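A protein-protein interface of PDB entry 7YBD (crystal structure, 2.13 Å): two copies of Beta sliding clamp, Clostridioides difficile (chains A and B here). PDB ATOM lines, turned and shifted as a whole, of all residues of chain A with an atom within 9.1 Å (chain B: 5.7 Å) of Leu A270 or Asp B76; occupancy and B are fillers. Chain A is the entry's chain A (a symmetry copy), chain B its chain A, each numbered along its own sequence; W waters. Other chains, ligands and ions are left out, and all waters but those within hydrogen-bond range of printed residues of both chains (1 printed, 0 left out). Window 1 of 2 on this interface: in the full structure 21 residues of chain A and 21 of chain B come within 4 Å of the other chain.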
ATOM      1  N   LEU A 262      11.309  -1.391 -12.775  1.00  0.00           N
ATOM      2  CA  LEU A 262      12.180  -2.397 -12.169  1.00  0.00           C
ATOM      3  C   LEU A 262      12.487  -3.517 -13.177  1.00  0.00           C
ATOM      4  O   LEU A 262      13.645  -3.852 -13.434  1.00  0.00           O
ATOM      5  CB  LEU A 262      11.507  -2.914 -10.885  1.00  0.00           C
ATOM      6  CG  LEU A 262      12.165  -4.110 -10.198  1.00  0.00           C
ATOM      7  CD1 LEU A 262      13.615  -3.856  -9.785  1.00  0.00           C
ATOM      8  CD2 LEU A 262      11.336  -4.560  -9.006  1.00  0.00           C
ATOM      9  N   ASN A 263      11.443  -4.073 -13.788  1.00  0.00           N
ATOM     10  CA  ASN A 263      11.593  -5.140 -14.772  1.00  0.00           C
ATOM     11  C   ASN A 263      12.527  -4.719 -15.909  1.00  0.00           C
ATOM     12  O   ASN A 263      13.411  -5.485 -16.291  1.00  0.00           O
ATOM     13  CB  ASN A 263      10.236  -5.566 -15.337  1.00  0.00           C
ATOM     14  CG  ASN A 263       9.384  -6.263 -14.301  1.00  0.00           C
ATOM     15  OD1 ASN A 263       9.895  -6.831 -13.343  1.00  0.00           O
ATOM     16  ND2 ASN A 263       8.081  -6.223 -14.488  1.00  0.00           N
ATOM     17  N   SER A 264      12.345  -3.495 -16.422  1.00  0.00           N
ATOM     18  CA  SER A 264      13.174  -2.955 -17.495  1.00  0.00           C
ATOM     19  C   SER A 264      14.620  -2.781 -17.046  1.00  0.00           C
ATOM     20  O   SER A 264      15.544  -3.157 -17.765  1.00  0.00           O
ATOM     21  CB  SER A 264      12.623  -1.661 -18.018  1.00  0.00           C
ATOM     22  OG  SER A 264      11.377  -1.900 -18.639  1.00  0.00           O
ATOM     23  N   ILE A 265      14.837  -2.213 -15.859  1.00  0.00           N
ATOM     24  CA  ILE A 265      16.219  -2.103 -15.421  1.00  0.00           C
ATOM     25  C   ILE A 265      16.835  -3.503 -15.269  1.00  0.00           C
ATOM     26  O   ILE A 265      17.945  -3.768 -15.747  1.00  0.00           O
ATOM     27  CB  ILE A 265      16.358  -1.168 -14.203  1.00  0.00           C
ATOM     28  CG1 ILE A 265      15.830   0.226 -14.577  1.00  0.00           C
ATOM     29  CG2 ILE A 265      17.814  -1.119 -13.743  1.00  0.00           C
ATOM     30  CD1 ILE A 265      15.903   1.266 -13.468  1.00  0.00           C
ATOM     31  N   GLU A 266      16.069  -4.436 -14.692  1.00  0.00           N
ATOM     32  CA  GLU A 266      16.573  -5.790 -14.523  1.00  0.00           C
ATOM     33  C   GLU A 266      17.006  -6.382 -15.862  1.00  0.00           C
ATOM     34  O   GLU A 266      18.078  -6.948 -15.965  1.00  0.00           O
ATOM     35  CB  GLU A 266      15.551  -6.680 -13.813  1.00  0.00           C
ATOM     36  CG  GLU A 266      15.616  -6.573 -12.301  1.00  0.00           C
ATOM     37  CD  GLU A 266      14.452  -7.267 -11.619  1.00  0.00           C
ATOM     38  OE1 GLU A 266      14.526  -7.469 -10.389  1.00  0.00           O
ATOM     39  OE2 GLU A 266      13.474  -7.630 -12.329  1.00  0.00           O
ATOM     40  N   ARG A 267      16.163  -6.271 -16.882  1.00  0.00           N
ATOM     41  CA  ARG A 267      16.516  -6.764 -18.203  1.00  0.00           C
ATOM     42  C   ARG A 267      17.755  -6.032 -18.733  1.00  0.00           C
ATOM     43  O   ARG A 267      18.708  -6.670 -19.173  1.00  0.00           O
ATOM     44  CB  ARG A 267      15.280  -6.732 -19.113  1.00  0.00           C
ATOM     45  CG  ARG A 267      14.302  -7.862 -18.795  1.00  0.00           C
ATOM     46  CD  ARG A 267      13.177  -7.949 -19.803  1.00  0.00           C
ATOM     47  NE  ARG A 267      12.334  -6.765 -19.872  1.00  0.00           N
ATOM     48  CZ  ARG A 267      11.199  -6.603 -19.197  1.00  0.00           C
ATOM     49  NH1 ARG A 267      10.763  -7.544 -18.378  1.00  0.00           N
ATOM     50  NH2 ARG A 267      10.511  -5.486 -19.332  1.00  0.00           N
ATOM     51  N   ALA A 268      17.757  -4.692 -18.679  1.00  0.00           N
ATOM     52  CA  ALA A 268      18.857  -3.924 -19.235  1.00  0.00           C
ATOM     53  C   ALA A 268      20.149  -4.358 -18.555  1.00  0.00           C
ATOM     54  O   ALA A 268      21.192  -4.429 -19.204  1.00  0.00           O
ATOM     55  CB  ALA A 268      18.622  -2.418 -19.109  1.00  0.00           C
ATOM     56  N   SER A 269      20.062  -4.703 -17.261  1.00  0.00           N
ATOM     57  CA  SER A 269      21.266  -4.960 -16.502  1.00  0.00           C
ATOM     58  C   SER A 269      21.846  -6.332 -16.828  1.00  0.00           C
ATOM     59  O   SER A 269      23.004  -6.617 -16.510  1.00  0.00           O
ATOM     60  CB  SER A 269      21.043  -4.788 -15.039  1.00  0.00           C
ATOM     61  OG  SER A 269      20.479  -5.962 -14.493  1.00  0.00           O
ATOM     62  N   LEU A 270      21.058  -7.187 -17.474  1.00  0.00           N
ATOM     63  CA  LEU A 270      21.617  -8.483 -17.840  1.00  0.00           C
ATOM     64  C   LEU A 270      22.877  -8.320 -18.690  1.00  0.00           C
ATOM     65  O   LEU A 270      23.784  -9.130 -18.604  1.00  0.00           O
ATOM     66  CB  LEU A 270      20.549  -9.347 -18.527  1.00  0.00           C
ATOM     67  CG  LEU A 270      19.380  -9.750 -17.621  1.00  0.00           C
ATOM     68  CD1 LEU A 270      18.234 -10.348 -18.427  1.00  0.00           C
ATOM     69  CD2 LEU A 270      19.831 -10.705 -16.511  1.00  0.00           C
ATOM     70  N   LEU A 271      22.972  -7.260 -19.486  1.00  0.00           N
ATOM     71  CA  LEU A 271      24.159  -7.096 -20.313  1.00  0.00           C
ATOM     72  C   LEU A 271      25.327  -6.433 -19.569  1.00  0.00           C
ATOM     73  O   LEU A 271      26.476  -6.725 -19.895  1.00  0.00           O
ATOM     74  CB  LEU A 271      23.804  -6.331 -21.588  1.00  0.00           C
ATOM     75  CG  LEU A 271      22.775  -7.023 -22.475  1.00  0.00           C
ATOM     76  CD1 LEU A 271      22.692  -6.310 -23.803  1.00  0.00           C
ATOM     77  CD2 LEU A 271      23.100  -8.500 -22.683  1.00  0.00           C
ATOM     78  N   SER A 272      25.058  -5.531 -18.610  1.00  0.00           N
ATOM     79  CA  SER A 272      26.125  -4.660 -18.108  1.00  0.00           C
ATOM     80  C   SER A 272      26.844  -5.241 -16.890  1.00  0.00           C
ATOM     81  O   SER A 272      27.726  -4.587 -16.327  1.00  0.00           O
ATOM     82  CB  SER A 272      25.708  -3.192 -17.906  1.00  0.00           C
ATOM     83  OG  SER A 272      24.445  -3.053 -17.271  1.00  0.00           O
ATOM     84  N   GLN A 273      26.464  -6.472 -16.521  1.00  0.00           N
ATOM     85  CA  GLN A 273      26.992  -7.186 -15.371  1.00  0.00           C
ATOM     86  C   GLN A 273      28.509  -7.368 -15.517  1.00  0.00           C
ATOM     87  O   GLN A 273      29.211  -7.086 -14.527  1.00  0.00           O
ATOM     88  CB  GLN A 273      26.292  -8.539 -15.249  1.00  0.00           C
ATOM     89  CG  GLN A 273      24.914  -8.454 -14.606  1.00  0.00           C
ATOM     90  CD  GLN A 273      24.161  -9.761 -14.697  1.00  0.00           C
ATOM     91  OE1 GLN A 273      24.393 -10.578 -15.592  1.00  0.00           O
ATOM     92  NE2 GLN A 273      23.240  -9.965 -13.765  1.00  0.00           N
ATOM     93  N   ASN A 278      27.929  -1.967 -13.910  1.00  0.00           N
ATOM     94  CA  ASN A 278      26.499  -2.250 -13.980  1.00  0.00           C
ATOM     95  C   ASN A 278      25.701  -1.145 -14.680  1.00  0.00           C
ATOM     96  O   ASN A 278      24.533  -0.980 -14.358  1.00  0.00           O
ATOM     97  CB  ASN A 278      25.891  -2.529 -12.598  1.00  0.00           C
ATOM     98  CG  ASN A 278      26.348  -3.822 -11.957  1.00  0.00           C
ATOM     99  OD1 ASN A 278      25.909  -4.901 -12.349  1.00  0.00           O
ATOM    100  ND2 ASN A 278      27.209  -3.722 -10.956  1.00  0.00           N
ATOM    101  N   LEU A 279      26.293  -0.431 -15.652  1.00  0.00           N
ATOM    102  CA  LEU A 279      25.736   0.824 -16.144  1.00  0.00           C
ATOM    103  C   LEU A 279      24.430   0.634 -16.923  1.00  0.00           C
ATOM    104  O   LEU A 279      24.336  -0.270 -17.753  1.00  0.00           O
ATOM    105  CB  LEU A 279      26.746   1.486 -17.077  1.00  0.00           C
ATOM    106  CG  LEU A 279      26.721   3.002 -16.977  1.00  0.00           C
ATOM    107  CD1 LEU A 279      27.557   3.429 -15.781  1.00  0.00           C
ATOM    108  CD2 LEU A 279      27.197   3.672 -18.263  1.00  0.00           C
ATOM    109  N   ILE A 280      23.453   1.535 -16.700  1.00  0.00           N
ATOM    110  CA  ILE A 280      22.309   1.666 -17.600  1.00  0.00           C
ATOM    111  C   ILE A 280      22.070   3.141 -17.888  1.00  0.00           C
ATOM    112  O   ILE A 280      22.518   3.993 -17.135  1.00  0.00           O
ATOM    113  CB  ILE A 280      21.055   0.932 -17.081  1.00  0.00           C
ATOM    114  CG1 ILE A 280      20.630   1.424 -15.691  1.00  0.00           C
ATOM    115  CG2 ILE A 280      21.255  -0.588 -17.116  1.00  0.00           C
ATOM    116  CD1 ILE A 280      19.464   2.376 -15.704  1.00  0.00           C
ATOM    117  N   THR A 292      18.591   1.734 -21.587  1.00  0.00           N
ATOM    118  CA  THR A 292      19.478   1.033 -22.491  1.00  0.00           C
ATOM    119  C   THR A 292      20.794   0.689 -21.812  1.00  0.00           C
ATOM    120  O   THR A 292      21.217   1.321 -20.834  1.00  0.00           O
ATOM    121  CB  THR A 292      19.770   1.839 -23.764  1.00  0.00           C
ATOM    122  OG1 THR A 292      20.467   3.030 -23.401  1.00  0.00           O
ATOM    123  CG2 THR A 292      18.520   2.211 -24.526  1.00  0.00           C
ATOM    124  N   SER A 293      21.426  -0.348 -22.374  1.00  0.00           N
ATOM    125  CA  SER A 293      22.815  -0.651 -22.092  1.00  0.00           C
ATOM    126  C   SER A 293      23.464  -1.199 -23.356  1.00  0.00           C
ATOM    127  O   SER A 293      22.790  -1.765 -24.222  1.00  0.00           O
ATOM    128  CB  SER A 293      22.963  -1.603 -20.937  1.00  0.00           C
ATOM    129  OG  SER A 293      22.201  -2.776 -21.180  1.00  0.00           O
ATOM    130  N   ASN A 294      24.777  -0.972 -23.444  1.00  0.00           N
ATOM    131  CA  ASN A 294      25.615  -1.349 -24.564  1.00  0.00           C
ATOM    132  C   ASN A 294      26.915  -1.839 -23.974  1.00  0.00           C
ATOM    133  O   ASN A 294      27.627  -1.084 -23.319  1.00  0.00           O
ATOM    134  CB  ASN A 294      26.102  -0.163 -25.385  1.00  0.00           C
ATOM    135  CG  ASN A 294      25.014   0.440 -26.224  1.00  0.00           C
ATOM    136  OD1 ASN A 294      25.121   0.442 -27.443  1.00  0.00           O
ATOM    137  ND2 ASN A 294      23.970   0.943 -25.586  1.00  0.00           N
ATOM    138  N   THR A 295      27.137  -3.128 -24.146  1.00  0.00           N
ATOM    139  CA  THR A 295      28.414  -3.743 -23.876  1.00  0.00           C
ATOM    140  C   THR A 295      28.820  -4.461 -25.158  1.00  0.00           C
ATOM    141  O   THR A 295      28.119  -4.421 -26.173  1.00  0.00           O
ATOM    142  CB  THR A 295      28.323  -4.628 -22.628  1.00  0.00           C
ATOM    143  OG1 THR A 295      27.498  -5.760 -22.901  1.00  0.00           O
ATOM    144  CG2 THR A 295      27.759  -3.896 -21.434  1.00  0.00           C
ATOM    145  N   LYS A 297      29.059  -7.425 -25.161  1.00  0.00           N
ATOM    146  CA  LYS A 297      28.208  -8.585 -25.003  1.00  0.00           C
ATOM    147  C   LYS A 297      26.865  -8.382 -25.716  1.00  0.00           C
ATOM    148  O   LYS A 297      26.191  -9.352 -26.052  1.00  0.00           O
ATOM    149  CB  LYS A 297      27.995  -8.817 -23.510  1.00  0.00           C
ATOM    150  CG  LYS A 297      27.919 -10.280 -23.111  1.00  0.00           C
ATOM    151  CD  LYS A 297      27.691 -10.484 -21.643  1.00  0.00           C
ATOM    152  CE  LYS A 297      28.073 -11.890 -21.231  1.00  0.00           C
ATOM    153  NZ  LYS A 297      28.258 -11.996 -19.765  1.00  0.00           N
ATOM    154  N   GLY A 298      26.467  -7.122 -25.922  1.00  0.00           N
ATOM    155  CA  GLY A 298      25.274  -6.800 -26.689  1.00  0.00           C
ATOM    156  C   GLY A 298      24.657  -5.483 -26.229  1.00  0.00           C
ATOM    157  O   GLY A 298      25.224  -4.763 -25.405  1.00  0.00           O
ATOM    158  N   ASN A 299      23.467  -5.188 -26.752  1.00  0.00           N
ATOM    159  CA  ASN A 299      22.719  -4.056 -26.240  1.00  0.00           C
ATOM    160  C   ASN A 299      21.262  -4.433 -26.011  1.00  0.00           C
ATOM    161  O   ASN A 299      20.754  -5.423 -26.552  1.00  0.00           O
ATOM    162  CB  ASN A 299      22.865  -2.796 -27.091  1.00  0.00           C
ATOM    163  CG  ASN A 299      22.813  -3.077 -28.572  1.00  0.00           C
ATOM    164  OD1 ASN A 299      23.852  -3.168 -29.220  1.00  0.00           O
ATOM    165  ND2 ASN A 299      21.621  -3.249 -29.104  1.00  0.00           N
ATOM    166  N   VAL A 300      20.632  -3.592 -25.196  1.00  0.00           N
ATOM    167  CA  VAL A 300      19.258  -3.723 -24.755  1.00  0.00           C
ATOM    168  C   VAL A 300      18.630  -2.357 -24.961  1.00  0.00           C
ATOM    169  O   VAL A 300      19.214  -1.348 -24.595  1.00  0.00           O
ATOM    170  CB  VAL A 300      19.159  -4.101 -23.260  1.00  0.00           C
ATOM    171  CG1 VAL A 300      17.716  -4.271 -22.839  1.00  0.00           C
ATOM    172  CG2 VAL A 300      19.896  -5.386 -22.967  1.00  0.00           C
ATOM    173  N   GLU A 302      14.956  -0.858 -23.767  1.00  0.00           N
ATOM    174  CA  GLU A 302      13.697  -1.118 -23.084  1.00  0.00           C
ATOM    175  C   GLU A 302      12.914   0.176 -23.160  1.00  0.00           C
ATOM    176  O   GLU A 302      13.530   1.240 -23.147  1.00  0.00           O
ATOM    177  CB  GLU A 302      13.942  -1.426 -21.600  1.00  0.00           C
ATOM    178  CG  GLU A 302      14.454  -2.834 -21.305  1.00  0.00           C
ATOM    179  CD  GLU A 302      13.384  -3.923 -21.299  1.00  0.00           C
ATOM    180  OE1 GLU A 302      13.713  -5.057 -21.735  1.00  0.00           O
ATOM    181  OE2 GLU A 302      12.224  -3.654 -20.861  1.00  0.00           O
ATOM    182  N   SER A 319      22.965   0.117 -12.104  1.00  0.00           N
ATOM    183  CA  SER A 319      21.701  -0.602 -12.144  1.00  0.00           C
ATOM    184  C   SER A 319      21.397  -1.256 -10.801  1.00  0.00           C
ATOM    185  O   SER A 319      20.229  -1.343 -10.430  1.00  0.00           O
ATOM    186  CB  SER A 319      21.614  -1.595 -13.285  1.00  0.00           C
ATOM    187  OG  SER A 319      22.692  -2.509 -13.230  1.00  0.00           O
ATOM    188  N   ILE A 323      17.980  -0.839  -8.909  1.00  0.00           N
ATOM    189  CA  ILE A 323      17.187  -2.028  -8.622  1.00  0.00           C
ATOM    190  C   ILE A 323      16.914  -2.136  -7.121  1.00  0.00           C
ATOM    191  O   ILE A 323      15.775  -2.368  -6.719  1.00  0.00           O
ATOM    192  CB  ILE A 323      17.848  -3.288  -9.230  1.00  0.00           C
ATOM    193  CG1 ILE A 323      17.756  -3.263 -10.762  1.00  0.00           C
ATOM    194  CG2 ILE A 323      17.243  -4.565  -8.668  1.00  0.00           C
ATOM    195  CD1 ILE A 323      18.679  -4.248 -11.494  1.00  0.00           C
ATOM    196  N   GLN B  18      19.547 -26.585 -20.828  1.00  0.00           N
ATOM    197  CA  GLN B  18      20.590 -26.163 -19.907  1.00  0.00           C
ATOM    198  C   GLN B  18      21.141 -27.339 -19.111  1.00  0.00           C
ATOM    199  O   GLN B  18      22.301 -27.298 -18.728  1.00  0.00           O
ATOM    200  CB  GLN B  18      20.154 -25.044 -18.966  1.00  0.00           C
ATOM    201  CG  GLN B  18      20.429 -23.669 -19.545  1.00  0.00           C
ATOM    202  CD  GLN B  18      19.818 -22.513 -18.781  1.00  0.00           C
ATOM    203  OE1 GLN B  18      18.860 -22.666 -18.034  1.00  0.00           O
ATOM    204  NE2 GLN B  18      20.341 -21.315 -19.002  1.00  0.00           N
ATOM    205  N   ALA B  71      24.288 -20.225 -23.351  1.00  0.00           N
ATOM    206  CA  ALA B  71      23.132 -20.855 -22.754  1.00  0.00           C
ATOM    207  C   ALA B  71      22.720 -20.064 -21.509  1.00  0.00           C
ATOM    208  O   ALA B  71      21.541 -19.774 -21.296  1.00  0.00           O
ATOM    209  CB  ALA B  71      23.402 -22.330 -22.529  1.00  0.00           C
ATOM    210  N   ARG B  72      23.690 -19.570 -20.750  1.00  0.00           N
ATOM    211  CA  ARG B  72      23.306 -18.813 -19.567  1.00  0.00           C
ATOM    212  C   ARG B  72      22.656 -17.455 -19.889  1.00  0.00           C
ATOM    213  O   ARG B  72      21.639 -17.060 -19.311  1.00  0.00           O
ATOM    214  CB  ARG B  72      24.490 -18.647 -18.611  1.00  0.00           C
ATOM    215  CG  ARG B  72      24.067 -17.876 -17.373  1.00  0.00           C
ATOM    216  CD  ARG B  72      25.003 -17.898 -16.193  1.00  0.00           C
ATOM    217  NE  ARG B  72      24.264 -17.265 -15.108  1.00  0.00           N
ATOM    218  CZ  ARG B  72      24.715 -17.114 -13.870  1.00  0.00           C
ATOM    219  NH1 ARG B  72      25.919 -17.559 -13.535  1.00  0.00           N
ATOM    220  NH2 ARG B  72      23.955 -16.516 -12.970  1.00  0.00           N
ATOM    221  N   LEU B  73      23.263 -16.690 -20.788  1.00  0.00           N
ATOM    222  CA  LEU B  73      22.684 -15.409 -21.149  1.00  0.00           C
ATOM    223  C   LEU B  73      21.271 -15.584 -21.745  1.00  0.00           C
ATOM    224  O   LEU B  73      20.314 -14.903 -21.354  1.00  0.00           O
ATOM    225  CB  LEU B  73      23.659 -14.686 -22.084  1.00  0.00           C
ATOM    226  CG  LEU B  73      23.229 -13.270 -22.421  1.00  0.00           C
ATOM    227  CD1 LEU B  73      23.185 -12.443 -21.146  1.00  0.00           C
ATOM    228  CD2 LEU B  73      24.128 -12.651 -23.484  1.00  0.00           C
ATOM    229  N   PHE B  74      21.131 -16.550 -22.652  1.00  0.00           N
ATOM    230  CA  PHE B  74      19.871 -16.820 -23.318  1.00  0.00           C
ATOM    231  C   PHE B  74      18.771 -17.090 -22.290  1.00  0.00           C
ATOM    232  O   PHE B  74      17.717 -16.466 -22.313  1.00  0.00           O
ATOM    233  CB  PHE B  74      20.070 -17.971 -24.301  1.00  0.00           C
ATOM    234  CG  PHE B  74      18.910 -18.213 -25.237  1.00  0.00           C
ATOM    235  CD1 PHE B  74      18.293 -17.158 -25.899  1.00  0.00           C
ATOM    236  CD2 PHE B  74      18.440 -19.499 -25.459  1.00  0.00           C
ATOM    237  CE1 PHE B  74      17.228 -17.385 -26.764  1.00  0.00           C
ATOM    238  CE2 PHE B  74      17.373 -19.726 -26.322  1.00  0.00           C
ATOM    239  CZ  PHE B  74      16.770 -18.670 -26.978  1.00  0.00           C
ATOM    240  N   GLY B  75      19.044 -18.016 -21.369  1.00  0.00           N
ATOM    241  CA  GLY B  75      18.122 -18.310 -20.284  1.00  0.00           C
ATOM    242  C   GLY B  75      17.803 -17.076 -19.445  1.00  0.00           C
ATOM    243  O   GLY B  75      16.633 -16.836 -19.190  1.00  0.00           O
ATOM    244  N   ASP B  76      18.819 -16.306 -19.023  1.00  0.00           N
ATOM    245  CA  ASP B  76      18.571 -15.152 -18.160  1.00  0.00           C
ATOM    246  C   ASP B  76      17.663 -14.125 -18.842  1.00  0.00           C
ATOM    247  O   ASP B  76      16.825 -13.521 -18.175  1.00  0.00           O
ATOM    248  CB  ASP B  76      19.849 -14.461 -17.685  1.00  0.00           C
ATOM    249  CG  ASP B  76      20.645 -15.323 -16.712  1.00  0.00           C
ATOM    250  OD1 ASP B  76      20.108 -16.337 -16.256  1.00  0.00           O
ATOM    251  OD2 ASP B  76      21.805 -15.006 -16.472  1.00  0.00           O
ATOM    252  N   ILE B  77      17.807 -13.946 -20.165  1.00  0.00           N
ATOM    253  CA  ILE B  77      16.955 -13.003 -20.878  1.00  0.00           C
ATOM    254  C   ILE B  77      15.523 -13.539 -20.946  1.00  0.00           C
ATOM    255  O   ILE B  77      14.576 -12.847 -20.555  1.00  0.00           O
ATOM    256  CB  ILE B  77      17.522 -12.703 -22.288  1.00  0.00           C
ATOM    257  CG1 ILE B  77      18.786 -11.838 -22.205  1.00  0.00           C
ATOM    258  CG2 ILE B  77      16.452 -12.081 -23.186  1.00  0.00           C
ATOM    259  CD1 ILE B  77      19.644 -11.834 -23.466  1.00  0.00           C
ATOM    260  N   ILE B  78      15.365 -14.761 -21.480  1.00  0.00           N
ATOM    261  CA  ILE B  78      14.035 -15.269 -21.744  1.00  0.00           C
ATOM    262  C   ILE B  78      13.231 -15.352 -20.449  1.00  0.00           C
ATOM    263  O   ILE B  78      12.056 -14.986 -20.422  1.00  0.00           O
ATOM    264  CB  ILE B  78      14.061 -16.584 -22.556  1.00  0.00           C
ATOM    265  CG1 ILE B  78      14.753 -16.377 -23.908  1.00  0.00           C
ATOM    266  CG2 ILE B  78      12.634 -17.113 -22.727  1.00  0.00           C
ATOM    267  CD1 ILE B  78      14.186 -15.209 -24.726  1.00  0.00           C
ATOM    268  N   ARG B  79      13.889 -15.735 -19.355  1.00  0.00           N
ATOM    269  CA  ARG B  79      13.233 -15.896 -18.068  1.00  0.00           C
ATOM    270  C   ARG B  79      12.595 -14.584 -17.594  1.00  0.00           C
ATOM    271  O   ARG B  79      11.601 -14.632 -16.879  1.00  0.00           O
ATOM    272  CB  ARG B  79      14.310 -16.287 -17.054  1.00  0.00           C
ATOM    273  CG  ARG B  79      13.939 -17.366 -16.055  1.00  0.00           C
ATOM    274  CD  ARG B  79      15.218 -18.033 -15.574  1.00  0.00           C
ATOM    275  NE  ARG B  79      15.530 -19.228 -16.359  1.00  0.00           N
ATOM    276  CZ  ARG B  79      16.754 -19.566 -16.801  1.00  0.00           C
ATOM    277  NH1 ARG B  79      17.791 -18.775 -16.567  1.00  0.00           N
ATOM    278  NH2 ARG B  79      16.937 -20.688 -17.492  1.00  0.00           N
ATOM    279  N   LYS B  80      13.185 -13.417 -17.920  1.00  0.00           N
ATOM    280  CA  LYS B  80      12.700 -12.128 -17.428  1.00  0.00           C
ATOM    281  C   LYS B  80      11.703 -11.451 -18.379  1.00  0.00           C
ATOM    282  O   LYS B  80      11.265 -10.326 -18.103  1.00  0.00           O
ATOM    283  CB  LYS B  80      13.855 -11.133 -17.273  1.00  0.00           C
ATOM    284  CG  LYS B  80      14.782 -11.344 -16.086  1.00  0.00           C
ATOM    285  CD  LYS B  80      14.099 -11.121 -14.767  1.00  0.00           C
ATOM    286  CE  LYS B  80      15.054 -11.152 -13.599  1.00  0.00           C
ATOM    287  NZ  LYS B  80      15.077 -12.511 -13.011  1.00  0.00           N
ATOM    288  N   PHE B 105      16.666  -6.767 -27.553  1.00  0.00           N
ATOM    289  CA  PHE B 105      18.027  -7.145 -27.219  1.00  0.00           C
ATOM    290  C   PHE B 105      18.711  -7.485 -28.526  1.00  0.00           C
ATOM    291  O   PHE B 105      18.074  -7.975 -29.476  1.00  0.00           O
ATOM    292  CB  PHE B 105      18.043  -8.459 -26.445  1.00  0.00           C
ATOM    293  CG  PHE B 105      17.593  -8.326 -25.017  1.00  0.00           C
ATOM    294  CD1 PHE B 105      16.245  -8.257 -24.712  1.00  0.00           C
ATOM    295  CD2 PHE B 105      18.529  -8.254 -23.992  1.00  0.00           C
ATOM    296  CE1 PHE B 105      15.842  -8.122 -23.396  1.00  0.00           C
ATOM    297  CE2 PHE B 105      18.120  -8.135 -22.674  1.00  0.00           C
ATOM    298  CZ  PHE B 105      16.774  -8.068 -22.385  1.00  0.00           C
HETATM  299  O   HOH W   1      10.572  -9.689 -15.211  1.00  0.00           O
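The guanidinium group (NH1) of Arg A267 sits at hydrogen-bond distance from the backbone carbonyl oxygen (O) of Lys B80, 2.8 Å away.
The backbone carbonyl oxygen (O) of Leu A270 sits close to the side-chain amide oxygen (OE1) of Gln A273 (3.4 Å).
The side-chain carboxylate (OD1) of Asp B76 lies within salt-bridge range of the guanidinium group (NH1) of Arg B79 (3.4 Å).
NE of Arg B72 lies within salt-bridge range of OD2 of Asp B76 (3.6 Å).
The guanidinium group (NE) of Arg A267 is in salt-bridge range of the side-chain carboxylate (OE1) of Glu A302 (2.9 Å).
O of Ser A293 is in hydrogen-bond range of N of Val A300 (3.0 Å).
CZ of Phe B105 touches CB of Arg A267, at 3.8 Å.
Leu A270 touches Asp B76 (CD1 to O, 3.5 Å).
CD1 of Leu A270 touches CA of Ile B77 (3.8 Å).
Phe B105 touches Asn A299.
Phe B105 touches Val A300 (CE2 to CG2, 3.3 Å).
Leu A262 touches none of the printed residues of chain B.
Of the printed residues of chain B, Arg A267 touches Lys B80 (2.8 Å) and Phe B105 (3.8 Å).
Of the printed residues of chain B, Asn A299 touches Phe B105 (3.3 Å).
Of the printed residues of chain B, Val A300 touches Phe B105 (3.3 Å).
No residue of chain A comes within 4 Å of Gly B75.
Printed residues of chain A within 4 Å of Ile B77: Leu A270.
Of the printed residues of chain A, Phe B105 touches Arg A267, Asn A299 and Val A300.
The nearest residue of chain B that does not touch Leu A270 is Leu B73 (4.2 Å).
The nearest residue of chain A that does not touch Asp B76 is Gln A273 (5.2 Å).
The nearest printed residue of chain B that does not touch Arg A267 is Ile B77 (5.1 Å).
Hydrophobic or aromatic side chains of chain B that line the printed part of chain A: Phe B105.
Of the 26 printed residues of chain A, 4 touch a printed residue of chain B.
Hydrophobic or aromatic side chains of chain A that line the printed part of chain B: Leu A270 and Val A300.
Among the printed residues, no Asp or Glu carboxylate lies within 4 Å of a Lys or Arg side-chain nitrogen of the other chain.
No position is printed for both chains.
Water W1 lies within hydrogen-bond range of the backbone carbonyl oxygen (O) of Lys B80 (3.0 Å) and the side-chain amide oxygen (OD1) of Asn A263 (3.5 Å).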
